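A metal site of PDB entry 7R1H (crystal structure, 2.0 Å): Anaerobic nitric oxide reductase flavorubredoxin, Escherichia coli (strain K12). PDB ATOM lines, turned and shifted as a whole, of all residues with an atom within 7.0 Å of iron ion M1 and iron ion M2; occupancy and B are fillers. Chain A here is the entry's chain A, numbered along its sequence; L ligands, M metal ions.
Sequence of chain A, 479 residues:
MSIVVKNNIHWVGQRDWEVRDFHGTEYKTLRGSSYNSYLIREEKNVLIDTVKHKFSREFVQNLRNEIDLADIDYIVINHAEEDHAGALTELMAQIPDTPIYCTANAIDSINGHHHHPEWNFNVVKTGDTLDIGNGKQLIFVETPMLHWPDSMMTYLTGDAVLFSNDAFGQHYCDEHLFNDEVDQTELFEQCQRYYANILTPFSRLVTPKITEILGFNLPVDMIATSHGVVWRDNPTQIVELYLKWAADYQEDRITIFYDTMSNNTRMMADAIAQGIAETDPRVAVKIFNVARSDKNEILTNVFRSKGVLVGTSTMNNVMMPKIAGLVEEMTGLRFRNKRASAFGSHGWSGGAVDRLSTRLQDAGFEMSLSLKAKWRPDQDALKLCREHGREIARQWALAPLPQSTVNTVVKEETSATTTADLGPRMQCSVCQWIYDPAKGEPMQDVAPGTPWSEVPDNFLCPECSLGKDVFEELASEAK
NE2 of His 147 sits close to O2 of LG2 L2 (3.4 Å). O2 of LG2 L2 sits at hydrogen-bond distance from OH of Tyr 194.
The backbone carbonyl oxygen (O) of Ser 34 lies within hydrogen-bond range of a ring nitrogen (ND1) of His 227 (2.8 Å). A ring nitrogen (NE2) of His 84 lies close to the side-chain hydroxyl (OG) of Ser 226. A ring nitrogen (NE2) of His 23 is in hydrogen-bond range of the side-chain carboxylate of Glu 81, at 2.6 Å. N of His 147 lies within hydrogen-bond range of OG of Ser 151. The backbone NH (N) of Asp 166 sits at hydrogen-bond distance from the side-chain hydroxyl (OG) of Ser 226 (3.2 Å).
Of the 20 residues printed, 4 come within 4 Å of iron ion M1.
Four residues have an atom within 4 Å of iron ion M2: His 79, Glu 81, His 147 and Asp 166.
Iron ion M1 is bound by O1 of LIG L1 (2.0 Å), NE2 of His 84 (2.1 Å), NE2 of His 227 (2.1 Å), OD1 of Asp 166 (2.3 Å) and OD2 of Asp 83 (2.4 Å). Slightly farther from iron ion M1 lies O1 of LG2 L2 (2.7 Å).
Iron ion M2 is bound by OD2 of Asp 166 (2.0 Å), OE1 of Glu 81 (2.0 Å), O1 of LIG L1 (2.1 Å), NE2 of His 147 (2.2 Å) and NE2 of His 79 (2.4 Å). Iron ion M2 has five donor atoms within binding distance.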
ATOM      1  N   PHE A  22      -5.458 -15.818  30.972  1.00  0.00           N
ATOM      2  CA  PHE A  22      -6.622 -14.941  31.098  1.00  0.00           C
ATOM      3  C   PHE A  22      -7.891 -15.783  31.154  1.00  0.00           C
ATOM      4  O   PHE A  22      -7.958 -16.848  30.533  1.00  0.00           O
ATOM      5  CB  PHE A  22      -6.689 -13.944  29.932  1.00  0.00           C
ATOM      6  CG  PHE A  22      -6.284 -12.546  30.305  1.00  0.00           C
ATOM      7  CD1 PHE A  22      -4.942 -12.197  30.352  1.00  0.00           C
ATOM      8  CD2 PHE A  22      -7.233 -11.586  30.588  1.00  0.00           C
ATOM      9  CE1 PHE A  22      -4.561 -10.904  30.698  1.00  0.00           C
ATOM     10  CE2 PHE A  22      -6.862 -10.296  30.931  1.00  0.00           C
ATOM     11  CZ  PHE A  22      -5.519  -9.956  30.983  1.00  0.00           C
ATOM     12  N   HIS A  23      -8.894 -15.316  31.891  1.00  0.00           N
ATOM     13  CA  HIS A  23     -10.141 -16.046  32.053  1.00  0.00           C
ATOM     14  C   HIS A  23      -9.882 -17.460  32.555  1.00  0.00           C
ATOM     15  O   HIS A  23     -10.243 -18.446  31.904  1.00  0.00           O
ATOM     16  CB  HIS A  23     -10.914 -16.087  30.730  1.00  0.00           C
ATOM     17  CG  HIS A  23     -11.306 -14.731  30.219  1.00  0.00           C
ATOM     18  ND1 HIS A  23     -11.543 -14.484  28.885  1.00  0.00           N
ATOM     19  CD2 HIS A  23     -11.509 -13.561  30.864  1.00  0.00           C
ATOM     20  CE1 HIS A  23     -11.865 -13.215  28.723  1.00  0.00           C
ATOM     21  NE2 HIS A  23     -11.852 -12.631  29.909  1.00  0.00           N
ATOM     22  N   SER A  34      -1.119  -5.929  28.278  1.00  0.00           N
ATOM     23  CA  SER A  34      -1.072  -4.609  28.897  1.00  0.00           C
ATOM     24  C   SER A  34      -2.491  -4.158  29.194  1.00  0.00           C
ATOM     25  O   SER A  34      -3.441  -4.594  28.549  1.00  0.00           O
ATOM     26  CB  SER A  34      -0.356  -3.606  27.995  1.00  0.00           C
ATOM     27  OG  SER A  34      -1.055  -3.428  26.781  1.00  0.00           O
ATOM     28  N   TYR A  35      -2.634  -3.294  30.198  1.00  0.00           N
ATOM     29  CA  TYR A  35      -3.927  -2.752  30.545  1.00  0.00           C
ATOM     30  C   TYR A  35      -3.871  -1.250  30.374  1.00  0.00           C
ATOM     31  O   TYR A  35      -3.220  -0.546  31.141  1.00  0.00           O
ATOM     32  CB  TYR A  35      -4.319  -3.150  31.976  1.00  0.00           C
ATOM     33  CG  TYR A  35      -3.955  -4.580  32.255  1.00  0.00           C
ATOM     34  CD1 TYR A  35      -4.608  -5.615  31.590  1.00  0.00           C
ATOM     35  CD2 TYR A  35      -2.948  -4.910  33.153  1.00  0.00           C
ATOM     36  CE1 TYR A  35      -4.276  -6.934  31.827  1.00  0.00           C
ATOM     37  CE2 TYR A  35      -2.609  -6.223  33.401  1.00  0.00           C
ATOM     38  CZ  TYR A  35      -3.277  -7.230  32.728  1.00  0.00           C
ATOM     39  OH  TYR A  35      -2.945  -8.549  32.966  1.00  0.00           O
ATOM     40  N   HIS A  79     -16.060  -0.662  30.124  1.00  0.00           N
ATOM     41  CA  HIS A  79     -16.190  -2.103  30.249  1.00  0.00           C
ATOM     42  C   HIS A  79     -15.737  -2.498  31.641  1.00  0.00           C
ATOM     43  O   HIS A  79     -14.654  -2.118  32.069  1.00  0.00           O
ATOM     44  CB  HIS A  79     -15.362  -2.787  29.154  1.00  0.00           C
ATOM     45  CG  HIS A  79     -15.393  -4.288  29.193  1.00  0.00           C
ATOM     46  ND1 HIS A  79     -16.558  -5.003  29.354  1.00  0.00           N
ATOM     47  CD2 HIS A  79     -14.401  -5.199  29.066  1.00  0.00           C
ATOM     48  CE1 HIS A  79     -16.278  -6.298  29.337  1.00  0.00           C
ATOM     49  NE2 HIS A  79     -14.976  -6.437  29.161  1.00  0.00           N
ATOM     50  N   ALA A  80     -16.570  -3.247  32.352  1.00  0.00           N
ATOM     51  CA  ALA A  80     -16.328  -3.474  33.771  1.00  0.00           C
ATOM     52  C   ALA A  80     -15.707  -4.835  34.066  1.00  0.00           C
ATOM     53  O   ALA A  80     -15.795  -5.326  35.186  1.00  0.00           O
ATOM     54  CB  ALA A  80     -17.627  -3.319  34.550  1.00  0.00           C
ATOM     55  N   GLU A  81     -15.070  -5.445  33.075  1.00  0.00           N
ATOM     56  CA  GLU A  81     -14.358  -6.684  33.332  1.00  0.00           C
ATOM     57  C   GLU A  81     -13.156  -6.347  34.212  1.00  0.00           C
ATOM     58  O   GLU A  81     -12.604  -5.255  34.120  1.00  0.00           O
ATOM     59  CB  GLU A  81     -13.928  -7.375  32.034  1.00  0.00           C
ATOM     60  CG  GLU A  81     -13.450  -8.807  32.251  1.00  0.00           C
ATOM     61  CD  GLU A  81     -13.551  -9.661  31.011  1.00  0.00           C
ATOM     62  OE1 GLU A  81     -13.741  -9.124  29.906  1.00  0.00           O
ATOM     63  OE2 GLU A  81     -13.429 -10.901  31.144  1.00  0.00           O
ATOM     64  N   GLU A  82     -12.789  -7.283  35.085  1.00  0.00           N
ATOM     65  CA  GLU A  82     -11.809  -7.026  36.144  1.00  0.00           C
ATOM     66  C   GLU A  82     -10.472  -6.481  35.672  1.00  0.00           C
ATOM     67  O   GLU A  82      -9.782  -5.801  36.430  1.00  0.00           O
ATOM     68  CB  GLU A  82     -11.591  -8.303  36.963  1.00  0.00           C
ATOM     69  CG  GLU A  82     -10.130  -8.726  37.114  1.00  0.00           C
ATOM     70  CD  GLU A  82      -9.605  -9.478  35.904  1.00  0.00           C
ATOM     71  OE1 GLU A  82     -10.340  -9.557  34.896  1.00  0.00           O
ATOM     72  OE2 GLU A  82      -8.470 -10.000  35.969  1.00  0.00           O
ATOM     73  N   ASP A  83     -10.086  -6.782  34.438  1.00  0.00           N
ATOM     74  CA  ASP A  83      -8.795  -6.343  33.942  1.00  0.00           C
ATOM     75  C   ASP A  83      -8.791  -4.866  33.553  1.00  0.00           C
ATOM     76  O   ASP A  83      -7.745  -4.302  33.245  1.00  0.00           O
ATOM     77  CB  ASP A  83      -8.346  -7.206  32.746  1.00  0.00           C
ATOM     78  CG  ASP A  83      -9.379  -7.260  31.650  1.00  0.00           C
ATOM     79  OD1 ASP A  83     -10.577  -7.088  31.966  1.00  0.00           O
ATOM     80  OD2 ASP A  83      -9.004  -7.484  30.480  1.00  0.00           O
ATOM     81  N   HIS A  84      -9.970  -4.246  33.576  1.00  0.00           N
ATOM     82  CA  HIS A  84     -10.069  -2.819  33.256  1.00  0.00           C
ATOM     83  C   HIS A  84     -10.680  -2.017  34.397  1.00  0.00           C
ATOM     84  O   HIS A  84     -10.340  -0.855  34.603  1.00  0.00           O
ATOM     85  CB  HIS A  84     -10.882  -2.615  31.975  1.00  0.00           C
ATOM     86  CG  HIS A  84     -10.390  -3.440  30.825  1.00  0.00           C
ATOM     87  ND1 HIS A  84      -9.114  -3.324  30.315  1.00  0.00           N
ATOM     88  CD2 HIS A  84     -10.987  -4.420  30.106  1.00  0.00           C
ATOM     89  CE1 HIS A  84      -8.955  -4.179  29.325  1.00  0.00           C
ATOM     90  NE2 HIS A  84     -10.086  -4.858  29.177  1.00  0.00           N
ATOM     91  N   HIS A 147     -17.572  -7.020  23.992  1.00  0.00           N
ATOM     92  CA  HIS A 147     -18.146  -8.365  24.010  1.00  0.00           C
ATOM     93  C   HIS A 147     -19.052  -8.632  25.211  1.00  0.00           C
ATOM     94  O   HIS A 147     -19.552  -9.754  25.371  1.00  0.00           O
ATOM     95  CB  HIS A 147     -17.016  -9.401  23.972  1.00  0.00           C
ATOM     96  CG  HIS A 147     -16.092  -9.335  25.150  1.00  0.00           C
ATOM     97  ND1 HIS A 147     -16.197 -10.190  26.219  1.00  0.00           N
ATOM     98  CD2 HIS A 147     -15.061  -8.503  25.433  1.00  0.00           C
ATOM     99  CE1 HIS A 147     -15.265  -9.897  27.114  1.00  0.00           C
ATOM    100  NE2 HIS A 147     -14.567  -8.881  26.656  1.00  0.00           N
ATOM    101  N   TRP A 148     -19.263  -7.632  26.052  1.00  0.00           N
ATOM    102  CA  TRP A 148     -20.171  -7.760  27.196  1.00  0.00           C
ATOM    103  C   TRP A 148     -21.388  -6.865  27.036  1.00  0.00           C
ATOM    104  O   TRP A 148     -21.391  -5.960  26.208  1.00  0.00           O
ATOM    105  CB  TRP A 148     -19.459  -7.404  28.506  1.00  0.00           C
ATOM    106  CG  TRP A 148     -18.785  -8.562  29.191  1.00  0.00           C
ATOM    107  CD1 TRP A 148     -18.485  -9.775  28.649  1.00  0.00           C
ATOM    108  CD2 TRP A 148     -18.308  -8.598  30.534  1.00  0.00           C
ATOM    109  NE1 TRP A 148     -17.855 -10.575  29.577  1.00  0.00           N
ATOM    110  CE2 TRP A 148     -17.738  -9.866  30.753  1.00  0.00           C
ATOM    111  CE3 TRP A 148     -18.310  -7.674  31.596  1.00  0.00           C
ATOM    112  CZ2 TRP A 148     -17.177 -10.245  31.966  1.00  0.00           C
ATOM    113  CZ3 TRP A 148     -17.759  -8.054  32.806  1.00  0.00           C
ATOM    114  CH2 TRP A 148     -17.199  -9.329  32.990  1.00  0.00           C
ATOM    115  N   SER A 151     -20.435  -3.149  27.494  1.00  0.00           N
ATOM    116  CA  SER A 151     -19.387  -2.593  26.640  1.00  0.00           C
ATOM    117  C   SER A 151     -19.803  -1.326  25.893  1.00  0.00           C
ATOM    118  O   SER A 151     -20.917  -1.227  25.372  1.00  0.00           O
ATOM    119  CB  SER A 151     -18.928  -3.636  25.617  1.00  0.00           C
ATOM    120  OG  SER A 151     -18.401  -4.784  26.254  1.00  0.00           O
ATOM    121  N   ASN A 165     -11.813   0.373  24.093  1.00  0.00           N
ATOM    122  CA  ASN A 165     -11.662  -0.698  25.081  1.00  0.00           C
ATOM    123  C   ASN A 165     -11.169  -2.003  24.444  1.00  0.00           C
ATOM    124  O   ASN A 165     -10.188  -1.992  23.701  1.00  0.00           O
ATOM    125  CB  ASN A 165     -12.971  -0.920  25.828  1.00  0.00           C
ATOM    126  CG  ASN A 165     -12.770  -1.678  27.138  1.00  0.00           C
ATOM    127  OD1 ASN A 165     -12.970  -2.897  27.199  1.00  0.00           O
ATOM    128  ND2 ASN A 165     -12.366  -0.970  28.187  1.00  0.00           N
ATOM    129  N   ASP A 166     -11.849  -3.107  24.705  1.00  0.00           N
ATOM    130  CA  ASP A 166     -11.392  -4.424  24.249  1.00  0.00           C
ATOM    131  C   ASP A 166     -11.292  -4.533  22.722  1.00  0.00           C
ATOM    132  O   ASP A 166     -10.376  -5.168  22.198  1.00  0.00           O
ATOM    133  CB  ASP A 166     -12.324  -5.521  24.776  1.00  0.00           C
ATOM    134  CG  ASP A 166     -11.934  -6.006  26.154  1.00  0.00           C
ATOM    135  OD1 ASP A 166     -10.786  -5.764  26.567  1.00  0.00           O
ATOM    136  OD2 ASP A 166     -12.774  -6.625  26.834  1.00  0.00           O
ATOM    137  N   HIS A 171      -3.486  -8.975  23.148  1.00  0.00           N
ATOM    138  CA  HIS A 171      -2.589  -9.221  24.269  1.00  0.00           C
ATOM    139  C   HIS A 171      -1.164  -9.334  23.775  1.00  0.00           C
ATOM    140  O   HIS A 171      -0.710 -10.396  23.334  1.00  0.00           O
ATOM    141  CB  HIS A 171      -3.028 -10.474  25.044  1.00  0.00           C
ATOM    142  CG  HIS A 171      -4.385 -10.339  25.659  1.00  0.00           C
ATOM    143  ND1 HIS A 171      -4.646  -9.498  26.723  1.00  0.00           N
ATOM    144  CD2 HIS A 171      -5.566 -10.923  25.351  1.00  0.00           C
ATOM    145  CE1 HIS A 171      -5.919  -9.587  27.044  1.00  0.00           C
ATOM    146  NE2 HIS A 171      -6.506 -10.444  26.235  1.00  0.00           N
ATOM    147  N   TYR A 194      -6.897 -12.967  19.427  1.00  0.00           N
ATOM    148  CA  TYR A 194      -7.916 -12.381  20.288  1.00  0.00           C
ATOM    149  C   TYR A 194      -9.302 -12.475  19.667  1.00  0.00           C
ATOM    150  O   TYR A 194     -10.257 -12.912  20.322  1.00  0.00           O
ATOM    151  CB  TYR A 194      -7.570 -10.919  20.596  1.00  0.00           C
ATOM    152  CG  TYR A 194      -8.544 -10.293  21.572  1.00  0.00           C
ATOM    153  CD1 TYR A 194      -9.599  -9.501  21.123  1.00  0.00           C
ATOM    154  CD2 TYR A 194      -8.425 -10.514  22.931  1.00  0.00           C
ATOM    155  CE1 TYR A 194     -10.496  -8.935  22.016  1.00  0.00           C
ATOM    156  CE2 TYR A 194      -9.312  -9.955  23.831  1.00  0.00           C
ATOM    157  CZ  TYR A 194     -10.341  -9.167  23.370  1.00  0.00           C
ATOM    158  OH  TYR A 194     -11.225  -8.604  24.257  1.00  0.00           O
ATOM    159  N   ILE A 198     -12.262 -14.873  21.211  1.00  0.00           N
ATOM    160  CA  ILE A 198     -13.144 -14.037  22.037  1.00  0.00           C
ATOM    161  C   ILE A 198     -14.360 -13.499  21.288  1.00  0.00           C
ATOM    162  O   ILE A 198     -15.477 -13.584  21.771  1.00  0.00           O
ATOM    163  CB  ILE A 198     -12.375 -12.835  22.617  1.00  0.00           C
ATOM    164  CG1 ILE A 198     -11.199 -13.320  23.477  1.00  0.00           C
ATOM    165  CG2 ILE A 198     -13.307 -11.941  23.431  1.00  0.00           C
ATOM    166  CD1 ILE A 198     -11.596 -14.176  24.648  1.00  0.00           C
ATOM    167  N   SER A 226      -7.875  -0.948  25.095  1.00  0.00           N
ATOM    168  CA  SER A 226      -7.532  -1.265  26.479  1.00  0.00           C
ATOM    169  C   SER A 226      -6.461  -2.354  26.585  1.00  0.00           C
ATOM    170  O   SER A 226      -5.980  -2.642  27.677  1.00  0.00           O
ATOM    171  CB  SER A 226      -8.792  -1.691  27.238  1.00  0.00           C
ATOM    172  OG  SER A 226      -9.359  -2.862  26.671  1.00  0.00           O
ATOM    173  N   HIS A 227      -6.067  -2.930  25.452  1.00  0.00           N
ATOM    174  CA  HIS A 227      -5.007  -3.943  25.424  1.00  0.00           C
ATOM    175  C   HIS A 227      -4.025  -3.727  24.289  1.00  0.00           C
ATOM    176  O   HIS A 227      -4.412  -3.687  23.117  1.00  0.00           O
ATOM    177  CB  HIS A 227      -5.599  -5.349  25.279  1.00  0.00           C
ATOM    178  CG  HIS A 227      -6.344  -5.831  26.479  1.00  0.00           C
ATOM    179  ND1 HIS A 227      -5.735  -6.036  27.696  1.00  0.00           N
ATOM    180  CD2 HIS A 227      -7.643  -6.166  26.652  1.00  0.00           C
ATOM    181  CE1 HIS A 227      -6.624  -6.468  28.572  1.00  0.00           C
ATOM    182  NE2 HIS A 227      -7.791  -6.555  27.958  1.00  0.00           N
HETATM  183  O1  LIG L   1     -11.498  -7.587  29.124  1.00  0.00           O
HETATM  184  O1  LG2 L   2     -10.259  -9.362  27.493  1.00  0.00           O
HETATM  185  O2  LG2 L   2     -11.353  -9.848  27.299  1.00  0.00           O
HETATM  186  N1  LG3 L   3     -22.502 -14.550  31.403  1.00  0.00           N
HETATM  187  C1  LG3 L   3     -23.725 -14.995  30.954  1.00  0.00           C
HETATM  188  O1  LG3 L   3     -24.719 -14.854  31.665  1.00  0.00           O
HETATM  189  N2  LG3 L   3     -23.836 -15.608  29.722  1.00  0.00           N
HETATM  190  C2  LG3 L   3     -22.720 -15.772  28.927  1.00  0.00           C
HETATM  191  O2  LG3 L   3     -22.818 -16.307  27.826  1.00  0.00           O
HETATM  192  C3  LG3 L   3     -21.478 -15.315  29.376  1.00  0.00           C
HETATM  193  N3  LG3 L   3     -20.356 -15.473  28.592  1.00  0.00           N
HETATM  194  C4  LG3 L   3     -19.126 -15.013  29.047  1.00  0.00           C
HETATM  195  C5  LG3 L   3     -17.992 -15.173  28.257  1.00  0.00           C
HETATM  196  C6  LG3 L   3     -16.765 -14.718  28.725  1.00  0.00           C
HETATM  197  C7  LG3 L   3     -15.530 -14.878  27.878  1.00  0.00           C
HETATM  198  C8  LG3 L   3     -16.667 -14.111  29.967  1.00  0.00           C
HETATM  199  C9  LG3 L   3     -15.340 -13.613  30.463  1.00  0.00           C
HETATM  200  C10 LG3 L   3     -17.802 -13.951  30.758  1.00  0.00           C
HETATM  201  C11 LG3 L   3     -19.041 -14.404  30.295  1.00  0.00           C
HETATM  202  N4  LG3 L   3     -20.159 -14.259  31.076  1.00  0.00           N
HETATM  203  C12 LG3 L   3     -21.380 -14.708  30.618  1.00  0.00           C
HETATM  204  C13 LG3 L   3     -20.071 -13.596  32.427  1.00  0.00           C
HETATM  205  C14 LG3 L   3     -19.531 -14.548  33.489  1.00  0.00           C
HETATM  206  O3  LG3 L   3     -20.335 -15.713  33.558  1.00  0.00           O
HETATM  207  C15 LG3 L   3     -19.492 -13.845  34.838  1.00  0.00           C
HETATM  208  O4  LG3 L   3     -18.392 -12.943  34.855  1.00  0.00           O
HETATM  209  C16 LG3 L   3     -19.365 -14.826  36.007  1.00  0.00           C
HETATM  210  O5  LG3 L   3     -19.750 -14.165  37.196  1.00  0.00           O
HETATM  211  C17 LG3 L   3     -17.932 -15.328  36.162  1.00  0.00           C
HETATM  212  O6  LG3 L   3     -17.881 -16.488  36.967  1.00  0.00           O
HETATM  213  P1  LG3 L   3     -16.439 -17.091  37.362  1.00  0.00           P
HETATM  214  O7  LG3 L   3     -16.587 -18.174  38.409  1.00  0.00           O
HETATM  215  O8  LG3 L   3     -15.780 -17.643  36.129  1.00  0.00           O
HETATM  216  O9  LG3 L   3     -15.592 -15.987  37.960  1.00  0.00           O
HETATM  217 FE    FE M   1      -9.881  -6.789  28.363  1.00  0.00          FE
HETATM  218 FE    FE M   2     -13.377  -7.925  28.286  1.00  0.00          FE
